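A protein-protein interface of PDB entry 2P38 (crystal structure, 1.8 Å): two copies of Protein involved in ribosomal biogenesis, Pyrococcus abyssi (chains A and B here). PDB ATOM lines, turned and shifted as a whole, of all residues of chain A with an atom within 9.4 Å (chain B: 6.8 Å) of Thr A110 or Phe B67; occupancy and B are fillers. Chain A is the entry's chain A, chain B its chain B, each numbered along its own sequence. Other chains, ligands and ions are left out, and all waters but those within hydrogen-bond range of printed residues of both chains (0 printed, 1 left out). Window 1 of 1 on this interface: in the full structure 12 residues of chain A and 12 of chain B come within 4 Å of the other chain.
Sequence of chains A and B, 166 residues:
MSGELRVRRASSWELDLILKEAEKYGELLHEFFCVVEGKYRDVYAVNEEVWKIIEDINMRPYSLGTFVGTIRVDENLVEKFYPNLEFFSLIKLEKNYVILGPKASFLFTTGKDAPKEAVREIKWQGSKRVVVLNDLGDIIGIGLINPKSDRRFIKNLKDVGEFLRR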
ATOM      1  N   LEU A 100      10.318  14.629 -20.318  1.00  0.00           N
ATOM      2  CA  LEU A 100      11.571  15.282 -20.641  1.00  0.00           C
ATOM      3  C   LEU A 100      11.899  16.133 -19.450  1.00  0.00           C
ATOM      4  O   LEU A 100      10.986  16.560 -18.746  1.00  0.00           O
ATOM      5  CB  LEU A 100      11.396  16.187 -21.868  1.00  0.00           C
ATOM      6  CG  LEU A 100      10.990  15.539 -23.177  1.00  0.00           C
ATOM      7  CD1 LEU A 100      11.064  16.568 -24.297  1.00  0.00           C
ATOM      8  CD2 LEU A 100      11.937  14.319 -23.482  1.00  0.00           C
ATOM      9  N   PRO A 102      13.262  19.736 -17.810  1.00  0.00           N
ATOM     10  CA  PRO A 102      12.685  21.053 -18.048  1.00  0.00           C
ATOM     11  C   PRO A 102      13.376  21.782 -19.197  1.00  0.00           C
ATOM     12  O   PRO A 102      12.690  22.486 -19.926  1.00  0.00           O
ATOM     13  CB  PRO A 102      12.909  21.792 -16.723  1.00  0.00           C
ATOM     14  CG  PRO A 102      13.860  21.024 -15.984  1.00  0.00           C
ATOM     15  CD  PRO A 102      13.860  19.624 -16.460  1.00  0.00           C
ATOM     16  N   LYS A 103      14.706  21.642 -19.334  1.00  0.00           N
ATOM     17  CA  LYS A 103      15.400  22.343 -20.400  1.00  0.00           C
ATOM     18  C   LYS A 103      14.975  21.822 -21.729  1.00  0.00           C
ATOM     19  O   LYS A 103      14.602  22.590 -22.596  1.00  0.00           O
ATOM     20  CB  LYS A 103      16.918  22.234 -20.244  1.00  0.00           C
ATOM     21  CG  LYS A 103      17.439  23.140 -19.177  1.00  0.00           C
ATOM     22  CD  LYS A 103      18.982  23.094 -19.075  1.00  0.00           C
ATOM     23  CE  LYS A 103      19.407  22.040 -18.110  1.00  0.00           C
ATOM     24  NZ  LYS A 103      20.257  22.614 -17.011  1.00  0.00           N
ATOM     25  N   ALA A 104      15.039  20.509 -21.889  1.00  0.00           N
ATOM     26  CA  ALA A 104      14.605  19.852 -23.117  1.00  0.00           C
ATOM     27  C   ALA A 104      13.121  20.074 -23.362  1.00  0.00           C
ATOM     28  O   ALA A 104      12.705  20.176 -24.526  1.00  0.00           O
ATOM     29  CB  ALA A 104      14.889  18.385 -23.057  1.00  0.00           C
ATOM     30  N   SER A 105      12.331  20.115 -22.283  1.00  0.00           N
ATOM     31  CA  SER A 105      10.886  20.328 -22.428  1.00  0.00           C
ATOM     32  C   SER A 105      10.708  21.683 -23.065  1.00  0.00           C
ATOM     33  O   SER A 105       9.938  21.845 -24.004  1.00  0.00           O
ATOM     34  CB  SER A 105      10.194  20.387 -21.053  1.00  0.00           C
ATOM     35  OG  SER A 105      10.073  19.088 -20.536  1.00  0.00           O
ATOM     36  N   PHE A 106      11.353  22.678 -22.478  1.00  0.00           N
ATOM     37  CA  PHE A 106      11.239  24.005 -23.057  1.00  0.00           C
ATOM     38  C   PHE A 106      11.606  24.019 -24.534  1.00  0.00           C
ATOM     39  O   PHE A 106      10.844  24.511 -25.397  1.00  0.00           O
ATOM     40  CB  PHE A 106      12.038  25.038 -22.323  1.00  0.00           C
ATOM     41  CG  PHE A 106      11.935  26.364 -22.972  1.00  0.00           C
ATOM     42  CD1 PHE A 106      10.792  27.130 -22.785  1.00  0.00           C
ATOM     43  CD2 PHE A 106      12.919  26.819 -23.836  1.00  0.00           C
ATOM     44  CE1 PHE A 106      10.630  28.344 -23.423  1.00  0.00           C
ATOM     45  CE2 PHE A 106      12.765  28.049 -24.504  1.00  0.00           C
ATOM     46  CZ  PHE A 106      11.616  28.801 -24.290  1.00  0.00           C
ATOM     47  N   LEU A 107      12.780  23.485 -24.840  1.00  0.00           N
ATOM     48  CA  LEU A 107      13.199  23.467 -26.225  1.00  0.00           C
ATOM     49  C   LEU A 107      12.213  22.741 -27.103  1.00  0.00           C
ATOM     50  O   LEU A 107      11.982  23.163 -28.239  1.00  0.00           O
ATOM     51  CB  LEU A 107      14.604  22.885 -26.400  1.00  0.00           C
ATOM     52  CG  LEU A 107      15.623  23.800 -25.733  1.00  0.00           C
ATOM     53  CD1 LEU A 107      16.956  23.066 -25.710  1.00  0.00           C
ATOM     54  CD2 LEU A 107      15.774  25.109 -26.447  1.00  0.00           C
ATOM     55  N   PHE A 108      11.620  21.662 -26.592  1.00  0.00           N
ATOM     56  CA  PHE A 108      10.632  20.923 -27.365  1.00  0.00           C
ATOM     57  C   PHE A 108       9.462  21.830 -27.765  1.00  0.00           C
ATOM     58  O   PHE A 108       8.922  21.756 -28.905  1.00  0.00           O
ATOM     59  CB  PHE A 108      10.184  19.690 -26.580  1.00  0.00           C
ATOM     60  CG  PHE A 108       9.432  18.724 -27.408  1.00  0.00           C
ATOM     61  CD1 PHE A 108      10.101  17.717 -28.081  1.00  0.00           C
ATOM     62  CD2 PHE A 108       8.049  18.847 -27.546  1.00  0.00           C
ATOM     63  CE1 PHE A 108       9.417  16.830 -28.859  1.00  0.00           C
ATOM     64  CE2 PHE A 108       7.340  17.942 -28.337  1.00  0.00           C
ATOM     65  CZ  PHE A 108       8.044  16.942 -28.994  1.00  0.00           C
ATOM     66  N   THR A 109       9.077  22.709 -26.849  1.00  0.00           N
ATOM     67  CA  THR A 109       7.959  23.607 -27.140  1.00  0.00           C
ATOM     68  C   THR A 109       8.349  24.630 -28.190  1.00  0.00           C
ATOM     69  O   THR A 109       7.458  25.260 -28.759  1.00  0.00           O
ATOM     70  CB  THR A 109       7.441  24.343 -25.892  1.00  0.00           C
ATOM     71  OG1 THR A 109       8.427  25.291 -25.440  1.00  0.00           O
ATOM     72  CG2 THR A 109       7.195  23.372 -24.731  1.00  0.00           C
ATOM     73  N   THR A 110       9.646  24.811 -28.439  1.00  0.00           N
ATOM     74  CA  THR A 110      10.095  25.691 -29.551  1.00  0.00           C
ATOM     75  C   THR A 110      10.262  24.966 -30.897  1.00  0.00           C
ATOM     76  O   THR A 110      10.748  25.567 -31.873  1.00  0.00           O
ATOM     77  CB  THR A 110      11.382  26.475 -29.253  1.00  0.00           C
ATOM     78  OG1 THR A 110      12.518  25.598 -29.327  1.00  0.00           O
ATOM     79  CG2 THR A 110      11.435  27.059 -27.820  1.00  0.00           C
ATOM     80  N   GLY A 111       9.872  23.690 -30.928  1.00  0.00           N
ATOM     81  CA  GLY A 111       9.931  22.824 -32.103  1.00  0.00           C
ATOM     82  C   GLY A 111      11.178  21.950 -32.177  1.00  0.00           C
ATOM     83  O   GLY A 111      11.441  21.285 -33.195  1.00  0.00           O
ATOM     84  N   LYS A 112      11.954  21.917 -31.110  1.00  0.00           N
ATOM     85  CA  LYS A 112      13.209  21.169 -31.139  1.00  0.00           C
ATOM     86  C   LYS A 112      12.902  19.719 -30.832  1.00  0.00           C
ATOM     87  O   LYS A 112      11.948  19.411 -30.118  1.00  0.00           O
ATOM     88  CB  LYS A 112      14.205  21.718 -30.128  1.00  0.00           C
ATOM     89  CG  LYS A 112      14.664  23.142 -30.406  1.00  0.00           C
ATOM     90  CD  LYS A 112      14.833  23.387 -31.900  1.00  0.00           C
ATOM     91  CE  LYS A 112      15.209  24.850 -32.137  1.00  0.00           C
ATOM     92  NZ  LYS A 112      14.164  25.739 -31.540  1.00  0.00           N
ATOM     93  N   ASP A 113      13.702  18.831 -31.409  1.00  0.00           N
ATOM     94  CA  ASP A 113      13.659  17.437 -31.029  1.00  0.00           C
ATOM     95  C   ASP A 113      14.209  17.301 -29.614  1.00  0.00           C
ATOM     96  O   ASP A 113      14.817  18.224 -29.068  1.00  0.00           O
ATOM     97  CB  ASP A 113      14.533  16.634 -31.982  1.00  0.00           C
ATOM     98  CG  ASP A 113      14.058  16.692 -33.406  1.00  0.00           C
ATOM     99  OD1 ASP A 113      12.841  16.885 -33.671  1.00  0.00           O
ATOM    100  OD2 ASP A 113      14.868  16.481 -34.348  1.00  0.00           O
ATOM    101  N   ILE A 140       3.312  18.477 -23.652  1.00  0.00           N
ATOM    102  CA  ILE A 140       3.931  19.578 -24.394  1.00  0.00           C
ATOM    103  C   ILE A 140       3.950  19.302 -25.874  1.00  0.00           C
ATOM    104  O   ILE A 140       4.251  20.178 -26.686  1.00  0.00           O
ATOM    105  CB  ILE A 140       5.324  19.927 -23.892  1.00  0.00           C
ATOM    106  CG1 ILE A 140       6.289  18.710 -23.943  1.00  0.00           C
ATOM    107  CG2 ILE A 140       5.259  20.470 -22.505  1.00  0.00           C
ATOM    108  CD1 ILE A 140       7.746  19.144 -23.454  1.00  0.00           C
ATOM    109  N   GLY A 141       3.594  18.100 -26.256  1.00  0.00           N
ATOM    110  CA  GLY A 141       3.521  17.858 -27.684  1.00  0.00           C
ATOM    111  C   GLY A 141       3.522  16.390 -27.973  1.00  0.00           C
ATOM    112  O   GLY A 141       3.338  15.568 -27.093  1.00  0.00           O
ATOM    113  N   ASN A 156      10.438  15.947 -32.779  1.00  0.00           N
ATOM    114  CA  ASN A 156       9.297  16.844 -32.622  1.00  0.00           C
ATOM    115  C   ASN A 156       8.321  16.833 -33.785  1.00  0.00           C
ATOM    116  O   ASN A 156       8.704  17.158 -34.891  1.00  0.00           O
ATOM    117  CB  ASN A 156       9.792  18.278 -32.441  1.00  0.00           C
ATOM    118  CG  ASN A 156       8.726  19.172 -31.856  1.00  0.00           C
ATOM    119  OD1 ASN A 156       7.625  19.307 -32.411  1.00  0.00           O
ATOM    120  ND2 ASN A 156       9.027  19.763 -30.718  1.00  0.00           N
ATOM    121  N   LYS A 158       4.569  17.823 -33.062  1.00  0.00           N
ATOM    122  CA  LYS A 158       3.603  18.852 -32.653  1.00  0.00           C
ATOM    123  C   LYS A 158       3.996  19.307 -31.253  1.00  0.00           C
ATOM    124  O   LYS A 158       4.429  18.490 -30.444  1.00  0.00           O
ATOM    125  CB  LYS A 158       2.181  18.273 -32.620  1.00  0.00           C
ATOM    126  N   ASP A 159       3.867  20.599 -30.955  1.00  0.00           N
ATOM    127  CA  ASP A 159       4.189  21.061 -29.602  1.00  0.00           C
ATOM    128  C   ASP A 159       3.330  22.247 -29.183  1.00  0.00           C
ATOM    129  O   ASP A 159       2.490  22.697 -29.960  1.00  0.00           O
ATOM    130  CB  ASP A 159       5.690  21.394 -29.480  1.00  0.00           C
ATOM    131  N   ARG B  41      19.248  30.165 -36.009  1.00  0.00           N
ATOM    132  CA  ARG B  41      19.266  31.230 -35.043  1.00  0.00           C
ATOM    133  C   ARG B  41      17.841  31.457 -34.557  1.00  0.00           C
ATOM    134  O   ARG B  41      17.004  31.952 -35.306  1.00  0.00           O
ATOM    135  CB  ARG B  41      19.805  32.478 -35.717  1.00  0.00           C
ATOM    136  CG  ARG B  41      21.340  32.522 -35.666  1.00  0.00           C
ATOM    137  CD  ARG B  41      21.948  33.650 -36.506  1.00  0.00           C
ATOM    138  NE  ARG B  41      21.665  33.456 -37.919  1.00  0.00           N
ATOM    139  CZ  ARG B  41      21.740  34.431 -38.807  1.00  0.00           C
ATOM    140  NH1 ARG B  41      21.982  35.673 -38.401  1.00  0.00           N
ATOM    141  NH2 ARG B  41      21.517  34.173 -40.077  1.00  0.00           N
ATOM    142  N   ASP B  42      17.585  31.107 -33.301  1.00  0.00           N
ATOM    143  CA  ASP B  42      16.246  31.273 -32.764  1.00  0.00           C
ATOM    144  C   ASP B  42      16.187  32.577 -32.055  1.00  0.00           C
ATOM    145  O   ASP B  42      17.106  32.946 -31.348  1.00  0.00           O
ATOM    146  CB  ASP B  42      15.942  30.171 -31.762  1.00  0.00           C
ATOM    147  CG  ASP B  42      15.525  28.928 -32.411  1.00  0.00           C
ATOM    148  OD1 ASP B  42      15.241  28.907 -33.628  1.00  0.00           O
ATOM    149  OD2 ASP B  42      15.410  27.884 -31.764  1.00  0.00           O
ATOM    150  N   VAL B  43      15.077  33.278 -32.227  1.00  0.00           N
ATOM    151  CA  VAL B  43      14.949  34.626 -31.698  1.00  0.00           C
ATOM    152  C   VAL B  43      14.045  34.599 -30.494  1.00  0.00           C
ATOM    153  O   VAL B  43      12.970  33.999 -30.569  1.00  0.00           O
ATOM    154  CB  VAL B  43      14.375  35.589 -32.785  1.00  0.00           C
ATOM    155  CG1 VAL B  43      14.086  36.971 -32.221  1.00  0.00           C
ATOM    156  CG2 VAL B  43      15.337  35.644 -33.984  1.00  0.00           C
ATOM    157  N   TYR B  44      14.522  35.199 -29.410  1.00  0.00           N
ATOM    158  CA  TYR B  44      13.723  35.296 -28.180  1.00  0.00           C
ATOM    159  C   TYR B  44      13.444  36.726 -27.883  1.00  0.00           C
ATOM    160  O   TYR B  44      14.354  37.589 -27.924  1.00  0.00           O
ATOM    161  CB  TYR B  44      14.489  34.638 -27.015  1.00  0.00           C
ATOM    162  CG  TYR B  44      14.437  33.171 -27.107  1.00  0.00           C
ATOM    163  CD1 TYR B  44      15.201  32.479 -28.065  1.00  0.00           C
ATOM    164  CD2 TYR B  44      13.632  32.423 -26.219  1.00  0.00           C
ATOM    165  CE1 TYR B  44      15.139  31.105 -28.154  1.00  0.00           C
ATOM    166  CE2 TYR B  44      13.594  31.040 -26.284  1.00  0.00           C
ATOM    167  CZ  TYR B  44      14.327  30.383 -27.248  1.00  0.00           C
ATOM    168  OH  TYR B  44      14.267  29.018 -27.341  1.00  0.00           O
ATOM    169  N   ALA B  45      12.171  37.029 -27.608  1.00  0.00           N
ATOM    170  CA  ALA B  45      11.857  38.305 -27.026  1.00  0.00           C
ATOM    171  C   ALA B  45      12.180  38.188 -25.556  1.00  0.00           C
ATOM    172  O   ALA B  45      11.675  37.300 -24.878  1.00  0.00           O
ATOM    173  CB  ALA B  45      10.375  38.634 -27.250  1.00  0.00           C
ATOM    174  N   PRO B  61      17.952  28.767 -23.048  1.00  0.00           N
ATOM    175  CA  PRO B  61      16.709  29.240 -23.684  1.00  0.00           C
ATOM    176  C   PRO B  61      15.531  29.230 -22.716  1.00  0.00           C
ATOM    177  O   PRO B  61      14.758  30.195 -22.766  1.00  0.00           O
ATOM    178  CB  PRO B  61      16.498  28.225 -24.793  1.00  0.00           C
ATOM    179  CG  PRO B  61      17.944  27.939 -25.215  1.00  0.00           C
ATOM    180  CD  PRO B  61      18.634  27.752 -23.876  1.00  0.00           C
ATOM    181  N   GLY B  65      12.999  34.047 -22.083  1.00  0.00           N
ATOM    182  CA  GLY B  65      11.860  34.825 -22.482  1.00  0.00           C
ATOM    183  C   GLY B  65      11.095  34.034 -23.517  1.00  0.00           C
ATOM    184  O   GLY B  65      10.995  32.779 -23.456  1.00  0.00           O
ATOM    185  N   THR B  66      10.593  34.740 -24.513  1.00  0.00           N
ATOM    186  CA  THR B  66       9.622  34.139 -25.375  1.00  0.00           C
ATOM    187  C   THR B  66      10.215  33.872 -26.728  1.00  0.00           C
ATOM    188  O   THR B  66      10.711  34.779 -27.359  1.00  0.00           O
ATOM    189  CB  THR B  66       8.435  35.095 -25.555  1.00  0.00           C
ATOM    190  OG1 THR B  66       7.855  35.276 -24.261  1.00  0.00           O
ATOM    191  CG2 THR B  66       7.376  34.394 -26.386  1.00  0.00           C
ATOM    192  N   PHE B  67      10.170  32.615 -27.123  1.00  0.00           N
ATOM    193  CA  PHE B  67      10.598  32.257 -28.453  1.00  0.00           C
ATOM    194  C   PHE B  67       9.637  32.830 -29.486  1.00  0.00           C
ATOM    195  O   PHE B  67       8.437  32.583 -29.422  1.00  0.00           O
ATOM    196  CB  PHE B  67      10.661  30.742 -28.543  1.00  0.00           C
ATOM    197  CG  PHE B  67      10.887  30.239 -29.920  1.00  0.00           C
ATOM    198  CD1 PHE B  67      12.078  30.532 -30.593  1.00  0.00           C
ATOM    199  CD2 PHE B  67       9.934  29.487 -30.548  1.00  0.00           C
ATOM    200  CE1 PHE B  67      12.271  30.054 -31.877  1.00  0.00           C
ATOM    201  CE2 PHE B  67      10.110  29.025 -31.840  1.00  0.00           C
ATOM    202  CZ  PHE B  67      11.315  29.313 -32.500  1.00  0.00           C
ATOM    203  N   VAL B  68      10.169  33.604 -30.422  1.00  0.00           N
ATOM    204  CA  VAL B  68       9.321  34.291 -31.386  1.00  0.00           C
ATOM    205  C   VAL B  68       9.620  33.991 -32.818  1.00  0.00           C
ATOM    206  O   VAL B  68       8.976  34.495 -33.710  1.00  0.00           O
ATOM    207  CB  VAL B  68       9.258  35.806 -31.154  1.00  0.00           C
ATOM    208  CG1 VAL B  68       8.612  36.091 -29.749  1.00  0.00           C
ATOM    209  CG2 VAL B  68      10.642  36.484 -31.273  1.00  0.00           C
ATOM    210  N   GLY B  69      10.567  33.105 -33.047  1.00  0.00           N
ATOM    211  CA  GLY B  69      10.795  32.707 -34.417  1.00  0.00           C
ATOM    212  C   GLY B  69      12.268  32.458 -34.659  1.00  0.00           C
ATOM    213  O   GLY B  69      13.040  32.400 -33.741  1.00  0.00           O
ATOM    214  N   THR B  70      12.627  32.345 -35.935  1.00  0.00           N
ATOM    215  CA  THR B  70      13.933  31.868 -36.297  1.00  0.00           C
ATOM    216  C   THR B  70      14.436  32.658 -37.486  1.00  0.00           C
ATOM    217  O   THR B  70      13.660  33.033 -38.353  1.00  0.00           O
ATOM    218  CB  THR B  70      13.785  30.421 -36.712  1.00  0.00           C
ATOM    219  OG1 THR B  70      13.241  29.693 -35.602  1.00  0.00           O
ATOM    220  CG2 THR B  70      15.153  29.789 -36.879  1.00  0.00           C
ATOM    221  N   TYR B  82      11.769  34.498 -39.561  1.00  0.00           N
ATOM    222  CA  TYR B  82      10.507  33.773 -39.688  1.00  0.00           C
ATOM    223  C   TYR B  82       9.822  33.810 -38.329  1.00  0.00           C
ATOM    224  O   TYR B  82      10.193  33.075 -37.439  1.00  0.00           O
ATOM    225  CB  TYR B  82      10.770  32.317 -40.057  1.00  0.00           C
ATOM    226  CG  TYR B  82      11.358  32.145 -41.422  1.00  0.00           C
ATOM    227  CD1 TYR B  82      12.737  32.273 -41.641  1.00  0.00           C
ATOM    228  CD2 TYR B  82      10.537  31.861 -42.503  1.00  0.00           C
ATOM    229  CE1 TYR B  82      13.287  32.083 -42.939  1.00  0.00           C
ATOM    230  CE2 TYR B  82      11.057  31.676 -43.776  1.00  0.00           C
ATOM    231  CZ  TYR B  82      12.432  31.781 -43.990  1.00  0.00           C
ATOM    232  OH  TYR B  82      12.920  31.587 -45.281  1.00  0.00           O
ATOM    233  N   ASN B  84       7.046  33.223 -35.362  1.00  0.00           N
ATOM    234  CA  ASN B  84       5.931  32.368 -35.012  1.00  0.00           C
ATOM    235  C   ASN B  84       4.786  33.299 -34.629  1.00  0.00           C
ATOM    236  O   ASN B  84       4.943  34.503 -34.665  1.00  0.00           O
ATOM    237  CB  ASN B  84       6.323  31.370 -33.922  1.00  0.00           C
ATOM    238  CG  ASN B  84       6.638  32.033 -32.604  1.00  0.00           C
ATOM    239  OD1 ASN B  84       6.337  33.182 -32.395  1.00  0.00           O
ATOM    240  ND2 ASN B  84       7.246  31.274 -31.684  1.00  0.00           N
ATOM    241  N   GLU B  86       3.533  33.991 -31.870  1.00  0.00           N
ATOM    242  CA  GLU B  86       3.782  34.745 -30.657  1.00  0.00           C
ATOM    243  C   GLU B  86       4.478  36.055 -30.959  1.00  0.00           C
ATOM    244  O   GLU B  86       4.325  37.040 -30.241  1.00  0.00           O
ATOM    245  CB  GLU B  86       4.568  33.898 -29.647  1.00  0.00           C
ATOM    246  CG  GLU B  86       4.730  34.592 -28.324  1.00  0.00           C
ATOM    247  CD  GLU B  86       3.490  34.548 -27.440  1.00  0.00           C
ATOM    248  OE1 GLU B  86       2.604  33.697 -27.659  1.00  0.00           O
ATOM    249  OE2 GLU B  86       3.413  35.381 -26.513  1.00  0.00           O
ATOM    250  N   PHE B  87       5.270  36.069 -32.029  1.00  0.00           N
ATOM    251  CA  PHE B  87       5.921  37.289 -32.396  1.00  0.00           C
ATOM    252  C   PHE B  87       4.889  38.381 -32.585  1.00  0.00           C
ATOM    253  O   PHE B  87       5.137  39.546 -32.267  1.00  0.00           O
ATOM    254  CB  PHE B  87       6.653  37.102 -33.720  1.00  0.00           C
ATOM    255  CG  PHE B  87       7.407  38.336 -34.158  1.00  0.00           C
ATOM    256  CD1 PHE B  87       8.452  38.825 -33.399  1.00  0.00           C
ATOM    257  CD2 PHE B  87       7.035  39.017 -35.308  1.00  0.00           C
ATOM    258  CE1 PHE B  87       9.134  39.974 -33.791  1.00  0.00           C
ATOM    259  CE2 PHE B  87       7.707  40.162 -35.704  1.00  0.00           C
ATOM    260  CZ  PHE B  87       8.772  40.640 -34.921  1.00  0.00           C
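The side-chain amino group of Lys A112 is in salt-bridge range of the side-chain carboxylate of Asp B42 (2.5 Å).
The backbone carbonyl oxygen of Phe A106 is in hydrogen-bond range of the side-chain hydroxyl of Thr A109 (2.5 Å).
O of Leu A107 lies within hydrogen-bond range of OG1 of Thr A110 (2.7 Å).
The side-chain hydroxyl (OG1) of Thr A110 is in hydrogen-bond range of the side-chain amino group (NZ) of Lys A112, at 2.8 Å.
ND2 of Asn A156 is in hydrogen-bond range of O of Lys A112 (3.0 Å).
The side-chain carboxylate (OD1) of Asp B42 lies within hydrogen-bond range of the side-chain hydroxyl (OG1) of Thr B70, at 2.9 Å.
O of Phe B67 is in hydrogen-bond range of ND2 of Asn B84.
Phe A106 touches Tyr B44 (CE2 to OH, 3.4 Å).
Pro B61 touches Phe A106 (O to CE2, 3.4 Å).
Leu A107 touches Pro B61.
Tyr B44 touches Thr A110.
Thr A110 touches Phe B67 (O to CE2, 3.5 Å).
Thr A110 touches just these residues of chain B: Tyr B44 and Phe B67.
Of chain A, only Thr A110 (3.5 Å) comes within 4 Å of Phe B67.
Thr B66 touches none of the printed residues of chain A.
No residue of chain A comes within 4 Å of Gly B69.
Printed residues of chain A within 4 Å of Tyr B44: Phe A106 (3.4 Å) and Thr A110 (3.5 Å).
Of the printed residues of chain B, Lys A112 touches Asp B42.
Printed residues of chain A within 4 Å of Asp B42: Lys A112.
Printed residues of chain B within 4 Å of Phe A106: Tyr B44 (3.4 Å) and Pro B61 (3.4 Å).
Phe B87 touches none of the printed residues of chain A.
Gly A141 touches none of the printed residues of chain B.
The nearest residue of chain B that does not touch Thr A110 is Asp B42 (4.4 Å).
The nearest residue of chain A that does not touch Phe B67 is Lys A112 (4.7 Å).
Hydrophobic or aromatic side chains of chain A within 4 Å of the printed part of chain B: Phe A106 and Leu A107.
Among the printed residues, Asp or Glu carboxylates within 4 Å of a Lys or Arg side-chain nitrogen of the other chain: Lys A112 with Asp B42 (2.5 Å).
No position is printed for both chains.
Of the 6 pairs that touch across the chains among the printed residues, none has its exchanged pair printed and touching as well.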
